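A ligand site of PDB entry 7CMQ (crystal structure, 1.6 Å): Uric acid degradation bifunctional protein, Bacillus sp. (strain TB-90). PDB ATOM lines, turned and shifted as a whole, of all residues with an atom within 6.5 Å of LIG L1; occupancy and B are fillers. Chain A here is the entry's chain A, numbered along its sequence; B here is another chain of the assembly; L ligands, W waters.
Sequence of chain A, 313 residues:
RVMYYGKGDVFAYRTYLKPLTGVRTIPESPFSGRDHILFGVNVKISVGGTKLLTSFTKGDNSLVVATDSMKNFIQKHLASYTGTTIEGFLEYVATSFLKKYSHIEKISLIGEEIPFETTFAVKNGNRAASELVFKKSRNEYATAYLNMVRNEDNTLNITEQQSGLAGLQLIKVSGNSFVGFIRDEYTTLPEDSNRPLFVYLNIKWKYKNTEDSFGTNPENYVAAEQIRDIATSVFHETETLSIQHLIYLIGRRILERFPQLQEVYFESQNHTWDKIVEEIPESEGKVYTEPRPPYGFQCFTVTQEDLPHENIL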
ATOM      1  N   SER A 177       5.362   1.943 -21.977  1.00  0.00           N
ATOM      2  CA  SER A 177       6.500   1.249 -22.538  1.00  0.00           C
ATOM      3  C   SER A 177       7.022   2.006 -23.753  1.00  0.00           C
ATOM      4  O   SER A 177       6.304   2.773 -24.406  1.00  0.00           O
ATOM      5  CB  SER A 177       6.177  -0.202 -22.943  1.00  0.00           C
ATOM      6  OG  SER A 177       5.522  -0.267 -24.191  1.00  0.00           O
ATOM      7  N   PHE A 178       8.306   1.798 -24.032  1.00  0.00           N
ATOM      8  CA  PHE A 178       8.898   2.253 -25.296  1.00  0.00           C
ATOM      9  C   PHE A 178       9.887   1.161 -25.704  1.00  0.00           C
ATOM     10  O   PHE A 178      11.010   1.118 -25.215  1.00  0.00           O
ATOM     11  CB  PHE A 178       9.565   3.612 -25.185  1.00  0.00           C
ATOM     12  CG  PHE A 178       9.962   4.180 -26.552  1.00  0.00           C
ATOM     13  CD1 PHE A 178       9.011   4.314 -27.544  1.00  0.00           C
ATOM     14  CD2 PHE A 178      11.267   4.503 -26.832  1.00  0.00           C
ATOM     15  CE1 PHE A 178       9.332   4.779 -28.799  1.00  0.00           C
ATOM     16  CE2 PHE A 178      11.610   4.968 -28.092  1.00  0.00           C
ATOM     17  CZ  PHE A 178      10.642   5.118 -29.076  1.00  0.00           C
ATOM     18  N   PHE A 181      11.769  -0.037 -31.194  1.00  0.00           N
ATOM     19  CA  PHE A 181      12.305   0.967 -32.096  1.00  0.00           C
ATOM     20  C   PHE A 181      13.617   0.492 -32.723  1.00  0.00           C
ATOM     21  O   PHE A 181      14.208  -0.516 -32.356  1.00  0.00           O
ATOM     22  CB  PHE A 181      12.474   2.304 -31.351  1.00  0.00           C
ATOM     23  CG  PHE A 181      13.221   2.202 -30.039  1.00  0.00           C
ATOM     24  CD1 PHE A 181      14.581   2.398 -29.991  1.00  0.00           C
ATOM     25  CD2 PHE A 181      12.550   1.910 -28.841  1.00  0.00           C
ATOM     26  CE1 PHE A 181      15.275   2.313 -28.798  1.00  0.00           C
ATOM     27  CE2 PHE A 181      13.235   1.820 -27.643  1.00  0.00           C
ATOM     28  CZ  PHE A 181      14.602   2.024 -27.623  1.00  0.00           C
ATOM     29  N   LEU A 189      19.763   4.005 -26.567  1.00  0.00           N
ATOM     30  CA  LEU A 189      18.638   4.019 -25.619  1.00  0.00           C
ATOM     31  C   LEU A 189      18.167   2.599 -25.322  1.00  0.00           C
ATOM     32  O   LEU A 189      17.819   1.870 -26.243  1.00  0.00           O
ATOM     33  CB  LEU A 189      17.489   4.821 -26.189  1.00  0.00           C
ATOM     34  CG  LEU A 189      16.238   4.924 -25.328  1.00  0.00           C
ATOM     35  CD1 LEU A 189      16.519   5.880 -24.155  1.00  0.00           C
ATOM     36  CD2 LEU A 189      15.033   5.384 -26.145  1.00  0.00           C
ATOM     37  N   ARG A 195       8.203   2.678 -17.983  1.00  0.00           N
ATOM     38  CA  ARG A 195       8.835   3.950 -17.711  1.00  0.00           C
ATOM     39  C   ARG A 195       7.815   4.951 -17.162  1.00  0.00           C
ATOM     40  O   ARG A 195       6.615   4.837 -17.423  1.00  0.00           O
ATOM     41  CB  ARG A 195       9.440   4.508 -18.991  1.00  0.00           C
ATOM     42  CG  ARG A 195       8.412   4.780 -20.094  1.00  0.00           C
ATOM     43  CD  ARG A 195       9.082   5.436 -21.312  1.00  0.00           C
ATOM     44  NE  ARG A 195       8.122   5.787 -22.344  1.00  0.00           N
ATOM     45  CZ  ARG A 195       8.409   6.462 -23.473  1.00  0.00           C
ATOM     46  NH1 ARG A 195       9.645   6.862 -23.713  1.00  0.00           N
ATOM     47  NH2 ARG A 195       7.451   6.742 -24.327  1.00  0.00           N
ATOM     48  N   LEU A 197       6.565   7.893 -17.986  1.00  0.00           N
ATOM     49  CA  LEU A 197       6.520   8.831 -19.115  1.00  0.00           C
ATOM     50  C   LEU A 197       6.051  10.202 -18.630  1.00  0.00           C
ATOM     51  O   LEU A 197       4.984  10.329 -18.019  1.00  0.00           O
ATOM     52  CB  LEU A 197       5.582   8.299 -20.179  1.00  0.00           C
ATOM     53  CG  LEU A 197       5.277   9.226 -21.349  1.00  0.00           C
ATOM     54  CD1 LEU A 197       6.534   9.641 -22.054  1.00  0.00           C
ATOM     55  CD2 LEU A 197       4.333   8.494 -22.286  1.00  0.00           C
ATOM     56  N   LEU A 241       2.386   3.024 -25.561  1.00  0.00           N
ATOM     57  CA  LEU A 241       3.464   2.376 -26.297  1.00  0.00           C
ATOM     58  C   LEU A 241       4.476   3.362 -26.850  1.00  0.00           C
ATOM     59  O   LEU A 241       5.515   2.941 -27.352  1.00  0.00           O
ATOM     60  CB  LEU A 241       2.878   1.535 -27.444  1.00  0.00           C
ATOM     61  CG  LEU A 241       1.974   0.366 -27.039  1.00  0.00           C
ATOM     62  CD1 LEU A 241       1.273  -0.194 -28.274  1.00  0.00           C
ATOM     63  CD2 LEU A 241       2.731  -0.716 -26.286  1.00  0.00           C
ATOM     64  N   SER A 242       4.192   4.669 -26.755  1.00  0.00           N
ATOM     65  CA  SER A 242       5.031   5.776 -27.183  1.00  0.00           C
ATOM     66  C   SER A 242       4.200   7.026 -26.887  1.00  0.00           C
ATOM     67  O   SER A 242       2.995   6.924 -26.622  1.00  0.00           O
ATOM     68  CB  SER A 242       5.362   5.736 -28.672  1.00  0.00           C
ATOM     69  OG  SER A 242       4.163   5.853 -29.412  1.00  0.00           O
ATOM     70  N   ILE A 243       4.837   8.177 -26.957  1.00  0.00           N
ATOM     71  CA  ILE A 243       4.051   9.409 -26.913  1.00  0.00           C
ATOM     72  C   ILE A 243       3.174   9.520 -28.151  1.00  0.00           C
ATOM     73  O   ILE A 243       2.011   9.931 -28.086  1.00  0.00           O
ATOM     74  CB  ILE A 243       4.964  10.631 -26.769  1.00  0.00           C
ATOM     75  CG1 ILE A 243       5.686  10.631 -25.430  1.00  0.00           C
ATOM     76  CG2 ILE A 243       4.155  11.900 -26.883  1.00  0.00           C
ATOM     77  CD1 ILE A 243       6.852  11.621 -25.391  1.00  0.00           C
ATOM     78  N   GLN A 244       3.717   9.150 -29.306  1.00  0.00           N
ATOM     79  CA  GLN A 244       2.944   9.108 -30.546  1.00  0.00           C
ATOM     80  C   GLN A 244       1.624   8.364 -30.364  1.00  0.00           C
ATOM     81  O   GLN A 244       0.553   8.852 -30.753  1.00  0.00           O
ATOM     82  CB  GLN A 244       3.801   8.434 -31.631  1.00  0.00           C
ATOM     83  CG  GLN A 244       5.035   9.252 -32.085  1.00  0.00           C
ATOM     84  CD  GLN A 244       6.309   8.964 -31.297  1.00  0.00           C
ATOM     85  OE1 GLN A 244       6.282   8.740 -30.092  1.00  0.00           O
ATOM     86  NE2 GLN A 244       7.442   8.994 -31.985  1.00  0.00           N
ATOM     87  N   ASN A 270       8.888  15.083 -24.788  1.00  0.00           N
ATOM     88  CA  ASN A 270       9.286  14.057 -23.833  1.00  0.00           C
ATOM     89  C   ASN A 270      10.291  14.613 -22.832  1.00  0.00           C
ATOM     90  O   ASN A 270      11.349  15.135 -23.229  1.00  0.00           O
ATOM     91  CB  ASN A 270       9.879  12.872 -24.594  1.00  0.00           C
ATOM     92  CG  ASN A 270      10.110  11.636 -23.726  1.00  0.00           C
ATOM     93  OD1 ASN A 270      10.032  11.685 -22.486  1.00  0.00           O
ATOM     94  ND2 ASN A 270      10.387  10.521 -24.381  1.00  0.00           N
ATOM     95  N   GLY A 296      12.804  15.026 -26.748  1.00  0.00           N
ATOM     96  CA  GLY A 296      12.018  14.587 -27.881  1.00  0.00           C
ATOM     97  C   GLY A 296      10.734  15.385 -28.031  1.00  0.00           C
ATOM     98  O   GLY A 296      10.198  15.941 -27.064  1.00  0.00           O
ATOM     99  N   PHE A 297      10.231  15.452 -29.254  1.00  0.00           N
ATOM    100  CA  PHE A 297       8.960  16.100 -29.485  1.00  0.00           C
ATOM    101  C   PHE A 297       8.234  15.446 -30.648  1.00  0.00           C
ATOM    102  O   PHE A 297       8.827  14.731 -31.489  1.00  0.00           O
ATOM    103  CB  PHE A 297       9.111  17.618 -29.733  1.00  0.00           C
ATOM    104  CG  PHE A 297       9.850  17.965 -30.985  1.00  0.00           C
ATOM    105  CD1 PHE A 297       9.209  17.981 -32.194  1.00  0.00           C
ATOM    106  CD2 PHE A 297      11.209  18.283 -30.936  1.00  0.00           C
ATOM    107  CE1 PHE A 297       9.886  18.303 -33.351  1.00  0.00           C
ATOM    108  CE2 PHE A 297      11.883  18.592 -32.086  1.00  0.00           C
ATOM    109  CZ  PHE A 297      11.234  18.604 -33.292  1.00  0.00           C
ATOM    110  N   GLN A 298       6.915  15.651 -30.641  1.00  0.00           N
ATOM    111  CA  GLN A 298       5.996  15.103 -31.634  1.00  0.00           C
ATOM    112  C   GLN A 298       4.974  16.183 -32.002  1.00  0.00           C
ATOM    113  O   GLN A 298       4.577  17.014 -31.163  1.00  0.00           O
ATOM    114  CB  GLN A 298       5.261  13.874 -31.097  1.00  0.00           C
ATOM    115  CG  GLN A 298       6.170  12.699 -30.758  1.00  0.00           C
ATOM    116  CD  GLN A 298       6.914  12.867 -29.445  1.00  0.00           C
ATOM    117  OE1 GLN A 298       6.530  13.653 -28.577  1.00  0.00           O
ATOM    118  NE2 GLN A 298       7.984  12.090 -29.284  1.00  0.00           N
ATOM    119  N   TYR B   5       8.185  14.269 -35.969  1.00  0.00           N
ATOM    120  CA  TYR B   5       8.731  14.120 -34.618  1.00  0.00           C
ATOM    121  C   TYR B   5      10.227  14.355 -34.702  1.00  0.00           C
ATOM    122  O   TYR B   5      10.830  14.364 -35.787  1.00  0.00           O
ATOM    123  CB  TYR B   5       8.366  12.752 -33.999  1.00  0.00           C
ATOM    124  CG  TYR B   5       9.210  11.581 -34.436  1.00  0.00           C
ATOM    125  CD1 TYR B   5      10.002  10.903 -33.515  1.00  0.00           C
ATOM    126  CD2 TYR B   5       9.225  11.165 -35.740  1.00  0.00           C
ATOM    127  CE1 TYR B   5      10.790   9.828 -33.914  1.00  0.00           C
ATOM    128  CE2 TYR B   5       9.995  10.110 -36.154  1.00  0.00           C
ATOM    129  CZ  TYR B   5      10.781   9.465 -35.236  1.00  0.00           C
ATOM    130  OH  TYR B   5      11.557   8.419 -35.679  1.00  0.00           O
ATOM    131  N   GLY B   6      10.841  14.600 -33.548  1.00  0.00           N
ATOM    132  CA  GLY B   6      12.245  14.927 -33.572  1.00  0.00           C
ATOM    133  C   GLY B   6      12.823  15.162 -32.202  1.00  0.00           C
ATOM    134  O   GLY B   6      12.309  14.672 -31.191  1.00  0.00           O
ATOM    135  N   LYS B   7      13.930  15.905 -32.194  1.00  0.00           N
ATOM    136  CA  LYS B   7      14.718  16.169 -30.992  1.00  0.00           C
ATOM    137  C   LYS B   7      15.121  17.631 -30.985  1.00  0.00           C
ATOM    138  O   LYS B   7      15.608  18.153 -31.993  1.00  0.00           O
ATOM    139  CB  LYS B   7      15.936  15.260 -30.944  1.00  0.00           C
ATOM    140  CG  LYS B   7      16.712  15.237 -29.642  1.00  0.00           C
ATOM    141  CD  LYS B   7      15.833  14.721 -28.525  1.00  0.00           C
ATOM    142  CE  LYS B   7      16.366  13.406 -28.025  1.00  0.00           C
ATOM    143  NZ  LYS B   7      15.685  12.892 -26.803  1.00  0.00           N
ATOM    144  N   ASN B  61       6.429   0.665 -33.343  1.00  0.00           N
ATOM    145  CA  ASN B  61       7.677   1.415 -33.340  1.00  0.00           C
ATOM    146  C   ASN B  61       8.713   0.845 -34.304  1.00  0.00           C
ATOM    147  O   ASN B  61       9.868   1.299 -34.300  1.00  0.00           O
ATOM    148  CB  ASN B  61       8.237   1.457 -31.910  1.00  0.00           C
ATOM    149  CG  ASN B  61       7.357   2.270 -30.973  1.00  0.00           C
ATOM    150  OD1 ASN B  61       6.813   3.299 -31.373  1.00  0.00           O
ATOM    151  ND2 ASN B  61       7.205   1.803 -29.726  1.00  0.00           N
ATOM    152  N   VAL B  64      10.495   3.514 -36.119  1.00  0.00           N
ATOM    153  CA  VAL B  64      10.812   4.705 -35.323  1.00  0.00           C
ATOM    154  C   VAL B  64      12.316   4.746 -35.071  1.00  0.00           C
ATOM    155  O   VAL B  64      12.868   3.878 -34.386  1.00  0.00           O
ATOM    156  CB  VAL B  64      10.036   4.737 -33.998  1.00  0.00           C
ATOM    157  CG1 VAL B  64      10.589   5.853 -33.103  1.00  0.00           C
ATOM    158  CG2 VAL B  64       8.554   4.921 -34.244  1.00  0.00           C
ATOM    159  N   VAL B  65      12.974   5.761 -35.615  1.00  0.00           N
ATOM    160  CA  VAL B  65      14.281   6.174 -35.122  1.00  0.00           C
ATOM    161  C   VAL B  65      14.072   6.877 -33.787  1.00  0.00           C
ATOM    162  O   VAL B  65      13.332   7.869 -33.701  1.00  0.00           O
ATOM    163  CB  VAL B  65      14.978   7.090 -36.138  1.00  0.00           C
ATOM    164  CG1 VAL B  65      16.351   7.516 -35.623  1.00  0.00           C
ATOM    165  CG2 VAL B  65      15.055   6.377 -37.503  1.00  0.00           C
ATOM    166  N   ALA B  66      14.655   6.339 -32.719  1.00  0.00           N
ATOM    167  CA  ALA B  66      14.466   6.974 -31.414  1.00  0.00           C
ATOM    168  C   ALA B  66      14.980   8.413 -31.482  1.00  0.00           C
ATOM    169  O   ALA B  66      15.992   8.723 -32.120  1.00  0.00           O
ATOM    170  CB  ALA B  66      15.172   6.204 -30.316  1.00  0.00           C
ATOM    171  N   THR B  67      14.232   9.332 -30.864  1.00  0.00           N
ATOM    172  CA  THR B  67      14.713  10.717 -30.831  1.00  0.00           C
ATOM    173  C   THR B  67      16.070  10.786 -30.149  1.00  0.00           C
ATOM    174  O   THR B  67      16.930  11.595 -30.548  1.00  0.00           O
ATOM    175  CB  THR B  67      13.707  11.640 -30.160  1.00  0.00           C
ATOM    176  OG1 THR B  67      13.513  11.282 -28.784  1.00  0.00           O
ATOM    177  CG2 THR B  67      12.353  11.600 -30.880  1.00  0.00           C
ATOM    178  N   ASP B  68      16.304   9.921 -29.158  1.00  0.00           N
ATOM    179  CA  ASP B  68      17.625   9.839 -28.533  1.00  0.00           C
ATOM    180  C   ASP B  68      18.711   9.486 -29.542  1.00  0.00           C
ATOM    181  O   ASP B  68      19.828  10.009 -29.469  1.00  0.00           O
ATOM    182  CB  ASP B  68      17.581   8.794 -27.399  1.00  0.00           C
ATOM    183  CG  ASP B  68      18.849   8.739 -26.603  1.00  0.00           C
ATOM    184  OD1 ASP B  68      19.039   9.634 -25.729  1.00  0.00           O
ATOM    185  OD2 ASP B  68      19.670   7.848 -26.869  1.00  0.00           O
ATOM    186  N   SER B  69      18.407   8.582 -30.484  1.00  0.00           N
ATOM    187  CA  SER B  69      19.362   8.224 -31.513  1.00  0.00           C
ATOM    188  C   SER B  69      19.646   9.397 -32.451  1.00  0.00           C
ATOM    189  O   SER B  69      20.776   9.560 -32.928  1.00  0.00           O
ATOM    190  CB  SER B  69      18.862   7.014 -32.299  1.00  0.00           C
ATOM    191  OG  SER B  69      18.599   5.924 -31.382  1.00  0.00           O
HETATM  192  N1  LIG L   1       8.777   8.340 -28.639  1.00  0.00           N
HETATM  193  C1  LIG L   1       8.678   8.102 -27.319  1.00  0.00           C
HETATM  194  O1  LIG L   1       7.573   7.996 -26.829  1.00  0.00           O
HETATM  195  N2  LIG L   1       9.797   7.967 -26.584  1.00  0.00           N
HETATM  196  C2  LIG L   1      11.012   8.083 -27.163  1.00  0.00           C
HETATM  197  C3  LIG L   1      11.120   8.309 -28.503  1.00  0.00           C
HETATM  198  C4  LIG L   1       9.955   8.463 -29.235  1.00  0.00           C
HETATM  199  O2  LIG L   1       9.962   8.699 -30.395  1.00  0.00           O
HETATM  200  N3  LIG L   1      12.442   8.367 -28.801  1.00  0.00           N
HETATM  201  N4  LIG L   1      13.166   8.185 -27.672  1.00  0.00           N
HETATM  202  N5  LIG L   1      12.264   7.993 -26.663  1.00  0.00           N
HETATM  203  O1  LG2 L   2      11.298  11.160 -27.099  1.00  0.00           O
HETATM  204  O2  LG2 L   2      10.441  11.481 -27.704  1.00  0.00           O
HETATM  205  O   HOH W   1      12.896   7.751 -23.914  1.00  0.00           O
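The backbone NH (N) of Ile 243 is in hydrogen-bond range of an oxygen (O1) of LIG L1 (2.7 Å). An oxygen (O1) of LIG L1 lies within hydrogen-bond range of the guanidinium group of Arg 195. N of Thr 67 of chain B lies within hydrogen-bond range of N3 of LIG L1 (2.9 Å). N3 of LIG L1 lies within hydrogen-bond range of OG1 of Thr 67 of chain B, 3.1 Å away. The side-chain amide oxygen (OE1) of Gln 244 is in hydrogen-bond range of a nitrogen (N1) of LIG L1 (2.9 Å). A nitrogen (N2) of LIG L1 lies close to the side-chain amide nitrogen of Asn 270, at 3.4 Å. The side-chain hydroxyl of Thr 67 of chain B is in hydrogen-bond range of an oxygen (O1) of LG2 L2 (2.8 Å). The side-chain amide nitrogen (ND2) of Asn 270 sits at hydrogen-bond distance from an oxygen (O1) of LG2 L2 (2.9 Å). An oxygen (O2) of LG2 L2 lies within hydrogen-bond range of the side-chain amide nitrogen (NE2) of Gln 298 (3.0 Å).
N5 of LIG L1 sits close to O1 of LG2 L2 (3.3 Å).
The side-chain hydroxyl (OG1) of Thr 67 of chain B sits at hydrogen-bond distance from the side-chain amino group (NZ) of Lys 7 of chain B, at 3.4 Å. The backbone NH (N) of Gln 244 sits close to the side-chain hydroxyl (OG) of Ser 242 (3.3 Å). The backbone NH (N) of Asn 270 is in hydrogen-bond range of the backbone carbonyl oxygen (O) of Gly 296, at 2.8 Å. The side-chain hydroxyl (OH) of Tyr 5 of chain B is in hydrogen-bond range of the backbone carbonyl oxygen (O) of Val 65 of chain B (2.7 Å).
CZ of Phe 178 touches C3 of LIG L1, at 3.3 Å. Leu 189 touches LIG L1 (CD2 to N4, 3.7 Å). Ser 242 touches LIG L1 (CA to O1, 3.4 Å). Gln 298 touches LIG L1. Tyr 5 of chain B touches LIG L1. CG1 of Val 64 of chain B touches O2 of LIG L1 (3.98 Å). Ala 66 of chain B touches LIG L1. N of Asp 68 of chain B touches N4 of LIG L1, 3.9 Å away. Hydrophobic or aromatic side chains that line LIG L1: Phe 178, Leu 189, Ile 243, Tyr 5 of chain B, Val 64 of chain B and Ala 66 of chain B. Within 4 Å of LIG L1: Phe 178, Leu 189, Arg 195, Ser 242, Ile 243, Gln 244, Asn 270, Gln 298, Tyr 5 of chain B, Val 64 of chain B, Ala 66 of chain B, Thr 67 of chain B and Asp 68 of chain B. The nearest printed residue that does not touch LIG L1 is Val 65 of chain B (4.8 Å).
Water W1 bridges N5 of LIG L1 (2.8 Å) and NH1 of Arg 195 (3.4 Å).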
